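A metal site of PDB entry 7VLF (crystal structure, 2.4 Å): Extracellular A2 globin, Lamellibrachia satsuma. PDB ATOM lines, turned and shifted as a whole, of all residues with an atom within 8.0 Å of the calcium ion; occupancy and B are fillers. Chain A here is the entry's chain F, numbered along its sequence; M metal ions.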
ATOM      1  N   ALA A 102      12.986   9.978  23.134  1.00  0.00           N
ATOM      2  CA  ALA A 102      14.330   9.707  22.622  1.00  0.00           C
ATOM      3  C   ALA A 102      14.360   9.717  21.103  1.00  0.00           C
ATOM      4  O   ALA A 102      15.387  10.046  20.510  1.00  0.00           O
ATOM      5  CB  ALA A 102      14.842   8.376  23.152  1.00  0.00           C
ATOM      6  N   GLU A 103      13.244   9.349  20.453  1.00  0.00           N
ATOM      7  CA  GLU A 103      13.168   9.483  19.010  1.00  0.00           C
ATOM      8  C   GLU A 103      13.208  10.951  18.598  1.00  0.00           C
ATOM      9  O   GLU A 103      13.808  11.301  17.578  1.00  0.00           O
ATOM     10  CB  GLU A 103      11.908   8.800  18.481  1.00  0.00           C
ATOM     11  CG  GLU A 103      11.945   8.541  16.988  1.00  0.00           C
ATOM     12  CD  GLU A 103      13.068   7.605  16.601  1.00  0.00           C
ATOM     13  OE1 GLU A 103      13.049   6.426  17.017  1.00  0.00           O
ATOM     14  OE2 GLU A 103      13.996   8.049  15.888  1.00  0.00           O
ATOM     15  N   TYR A 105      14.868  13.101  20.186  1.00  0.00           N
ATOM     16  CA  TYR A 105      16.303  13.355  20.243  1.00  0.00           C
ATOM     17  C   TYR A 105      16.990  12.877  18.973  1.00  0.00           C
ATOM     18  O   TYR A 105      17.834  13.577  18.402  1.00  0.00           O
ATOM     19  CB  TYR A 105      16.926  12.672  21.467  1.00  0.00           C
ATOM     20  CG  TYR A 105      16.846  13.471  22.746  1.00  0.00           C
ATOM     21  CD1 TYR A 105      17.694  14.546  22.969  1.00  0.00           C
ATOM     22  CD2 TYR A 105      15.941  13.139  23.737  1.00  0.00           C
ATOM     23  CE1 TYR A 105      17.627  15.276  24.140  1.00  0.00           C
ATOM     24  CE2 TYR A 105      15.873  13.855  24.908  1.00  0.00           C
ATOM     25  CZ  TYR A 105      16.711  14.925  25.101  1.00  0.00           C
ATOM     26  OH  TYR A 105      16.631  15.641  26.280  1.00  0.00           O
ATOM     27  N   ASN A 106      16.642  11.669  18.516  1.00  0.00           N
ATOM     28  CA  ASN A 106      17.294  11.134  17.325  1.00  0.00           C
ATOM     29  C   ASN A 106      16.932  11.910  16.069  1.00  0.00           C
ATOM     30  O   ASN A 106      17.709  11.943  15.119  1.00  0.00           O
ATOM     31  CB  ASN A 106      16.948   9.655  17.160  1.00  0.00           C
ATOM     32  CG  ASN A 106      17.602   8.792  18.209  1.00  0.00           C
ATOM     33  OD1 ASN A 106      18.733   9.053  18.629  1.00  0.00           O
ATOM     34  ND2 ASN A 106      16.908   7.748  18.640  1.00  0.00           N
ATOM     35  N   VAL A 107      15.746  12.533  16.062  1.00  0.00           N
ATOM     36  CA  VAL A 107      15.340  13.302  14.881  1.00  0.00           C
ATOM     37  C   VAL A 107      16.156  14.579  14.768  1.00  0.00           C
ATOM     38  O   VAL A 107      16.676  14.919  13.704  1.00  0.00           O
ATOM     39  CB  VAL A 107      13.832  13.588  14.917  1.00  0.00           C
ATOM     40  CG1 VAL A 107      13.470  14.627  13.880  1.00  0.00           C
ATOM     41  CG2 VAL A 107      13.042  12.305  14.679  1.00  0.00           C
ATOM     42  N   GLU A 109      18.978  15.029  16.087  1.00  0.00           N
ATOM     43  CA  GLU A 109      20.319  14.548  15.778  1.00  0.00           C
ATOM     44  C   GLU A 109      20.536  14.512  14.279  1.00  0.00           C
ATOM     45  O   GLU A 109      21.472  15.121  13.750  1.00  0.00           O
ATOM     46  CB  GLU A 109      20.542  13.167  16.372  1.00  0.00           C
ATOM     47  CG  GLU A 109      20.865  13.131  17.852  1.00  0.00           C
ATOM     48  CD  GLU A 109      20.967  11.709  18.378  1.00  0.00           C
ATOM     49  OE1 GLU A 109      20.853  10.781  17.561  1.00  0.00           O
ATOM     50  OE2 GLU A 109      21.167  11.531  19.596  1.00  0.00           O
ATOM     51  N   HIS A 110      19.664  13.785  13.569  1.00  0.00           N
ATOM     52  CA  HIS A 110      19.739  13.734  12.124  1.00  0.00           C
ATOM     53  C   HIS A 110      19.523  15.109  11.502  1.00  0.00           C
ATOM     54  O   HIS A 110      20.082  15.398  10.434  1.00  0.00           O
ATOM     55  CB  HIS A 110      18.718  12.741  11.589  1.00  0.00           C
ATOM     56  CG  HIS A 110      18.677  12.641  10.097  1.00  0.00           C
ATOM     57  ND1 HIS A 110      17.807  13.382   9.321  1.00  0.00           N
ATOM     58  CD2 HIS A 110      19.401  11.896   9.240  1.00  0.00           C
ATOM     59  CE1 HIS A 110      18.001  13.094   8.047  1.00  0.00           C
ATOM     60  NE2 HIS A 110      18.962  12.194   7.969  1.00  0.00           N
ATOM     61  N   MET A 113      22.806  16.909  11.738  1.00  0.00           N
ATOM     62  CA  MET A 113      23.742  16.346  10.768  1.00  0.00           C
ATOM     63  C   MET A 113      23.433  16.798   9.351  1.00  0.00           C
ATOM     64  O   MET A 113      24.316  16.830   8.499  1.00  0.00           O
ATOM     65  CB  MET A 113      23.736  14.821  10.857  1.00  0.00           C
ATOM     66  CG  MET A 113      24.400  14.278  12.111  1.00  0.00           C
ATOM     67  SD  MET A 113      24.608  12.481  12.117  1.00  0.00           S
ATOM     68  CE  MET A 113      22.911  11.938  12.247  1.00  0.00           C
ATOM     69  N   GLN A 131      27.486  11.341  14.279  1.00  0.00           N
ATOM     70  CA  GLN A 131      26.427  10.484  14.813  1.00  0.00           C
ATOM     71  C   GLN A 131      26.835   9.873  16.157  1.00  0.00           C
ATOM     72  O   GLN A 131      25.996   9.724  17.057  1.00  0.00           O
ATOM     73  CB  GLN A 131      26.068   9.389  13.810  1.00  0.00           C
ATOM     74  CG  GLN A 131      25.070   8.360  14.318  1.00  0.00           C
ATOM     75  CD  GLN A 131      23.697   8.951  14.559  1.00  0.00           C
ATOM     76  OE1 GLN A 131      23.446   9.582  15.581  1.00  0.00           O
ATOM     77  NE2 GLN A 131      22.788   8.742  13.607  1.00  0.00           N
ATOM     78  N   ALA A 132      28.112   9.531  16.302  1.00  0.00           N
ATOM     79  CA  ALA A 132      28.578   8.970  17.563  1.00  0.00           C
ATOM     80  C   ALA A 132      28.606  10.015  18.669  1.00  0.00           C
ATOM     81  O   ALA A 132      28.179   9.753  19.797  1.00  0.00           O
ATOM     82  CB  ALA A 132      29.969   8.347  17.380  1.00  0.00           C
ATOM     83  N   LEU A 134      26.928  12.909  18.724  1.00  0.00           N
ATOM     84  CA  LEU A 134      25.596  13.441  19.006  1.00  0.00           C
ATOM     85  C   LEU A 134      24.846  12.555  19.994  1.00  0.00           C
ATOM     86  O   LEU A 134      24.132  13.066  20.867  1.00  0.00           O
ATOM     87  CB  LEU A 134      24.797  13.589  17.708  1.00  0.00           C
ATOM     88  CG  LEU A 134      25.126  14.786  16.819  1.00  0.00           C
ATOM     89  CD1 LEU A 134      24.167  14.854  15.643  1.00  0.00           C
ATOM     90  CD2 LEU A 134      25.082  16.084  17.618  1.00  0.00           C
ATOM     91  N   ASP A 135      25.004  11.239  19.883  1.00  0.00           N
ATOM     92  CA  ASP A 135      24.371  10.348  20.843  1.00  0.00           C
ATOM     93  C   ASP A 135      24.923  10.529  22.249  1.00  0.00           C
ATOM     94  O   ASP A 135      24.214  10.271  23.226  1.00  0.00           O
ATOM     95  CB  ASP A 135      24.536   8.892  20.398  1.00  0.00           C
ATOM     96  CG  ASP A 135      23.559   8.499  19.312  1.00  0.00           C
ATOM     97  OD1 ASP A 135      22.444   9.055  19.301  1.00  0.00           O
ATOM     98  OD2 ASP A 135      23.900   7.646  18.468  1.00  0.00           O
ATOM     99  N   VAL A 136      26.176  10.982  22.364  1.00  0.00           N
ATOM    100  CA  VAL A 136      26.737  11.257  23.687  1.00  0.00           C
ATOM    101  C   VAL A 136      26.080  12.502  24.281  1.00  0.00           C
ATOM    102  O   VAL A 136      25.719  12.518  25.468  1.00  0.00           O
ATOM    103  CB  VAL A 136      28.267  11.425  23.582  1.00  0.00           C
ATOM    104  CG1 VAL A 136      28.816  11.991  24.883  1.00  0.00           C
ATOM    105  CG2 VAL A 136      28.913  10.089  23.263  1.00  0.00           C
ATOM    106  N   THR A 138      23.080  13.832  23.472  1.00  0.00           N
ATOM    107  CA  THR A 138      21.670  13.575  23.756  1.00  0.00           C
ATOM    108  C   THR A 138      21.498  12.603  24.926  1.00  0.00           C
ATOM    109  O   THR A 138      20.518  12.707  25.671  1.00  0.00           O
ATOM    110  CB  THR A 138      20.975  13.029  22.514  1.00  0.00           C
ATOM    111  OG1 THR A 138      21.672  11.871  22.042  1.00  0.00           O
ATOM    112  CG2 THR A 138      20.951  14.079  21.427  1.00  0.00           C
ATOM    113  N   SER A 139      22.429  11.663  25.103  1.00  0.00           N
ATOM    114  CA  SER A 139      22.384  10.812  26.282  1.00  0.00           C
ATOM    115  C   SER A 139      22.537  11.627  27.556  1.00  0.00           C
ATOM    116  O   SER A 139      21.915  11.300  28.579  1.00  0.00           O
ATOM    117  CB  SER A 139      23.487   9.749  26.198  1.00  0.00           C
ATOM    118  OG  SER A 139      23.341   8.945  25.040  1.00  0.00           O
HETATM  119 CA    CA M   1      20.869   8.041  17.716  1.00  0.00          CA
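The backbone carbonyl oxygen (O) of Ala 102 sits at hydrogen-bond distance from the side-chain amide nitrogen (ND2) of Asn 106 (3.3 Å). The backbone carbonyl oxygen of Asp 135 lies within hydrogen-bond range of the side-chain hydroxyl of Thr 138 (3.2 Å). N of Gln 131 lies within hydrogen-bond range of SD of Met 113, 3.8 Å away. The side-chain carboxylate (OE1) of Glu 109 lies close to the side-chain amide oxygen (OE1) of Gln 131, at 3.5 Å. The side-chain hydroxyl (OG1) of Thr 138 sits at hydrogen-bond distance from the side-chain carboxylate (OE2) of Glu 109. The side-chain hydroxyl (OG) of Ser 139 lies within hydrogen-bond range of the backbone carbonyl oxygen (O) of Asp 135, at 2.4 Å.
Merely in contact with the calcium ion: Gln 131. Along chain A the residues within 4 Å of the calcium ion span positions 106 to 135. The nearest printed residue that does not touch the calcium ion is Thr 138 (5.8 Å).
The calcium ion is bound by OD1 of Asp 135, OD1 of Asn 106 and OE1 of Glu 109. Slightly farther from the calcium ion lies the side-chain carboxylate (OD2) of Asp 135 (3.1 Å).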
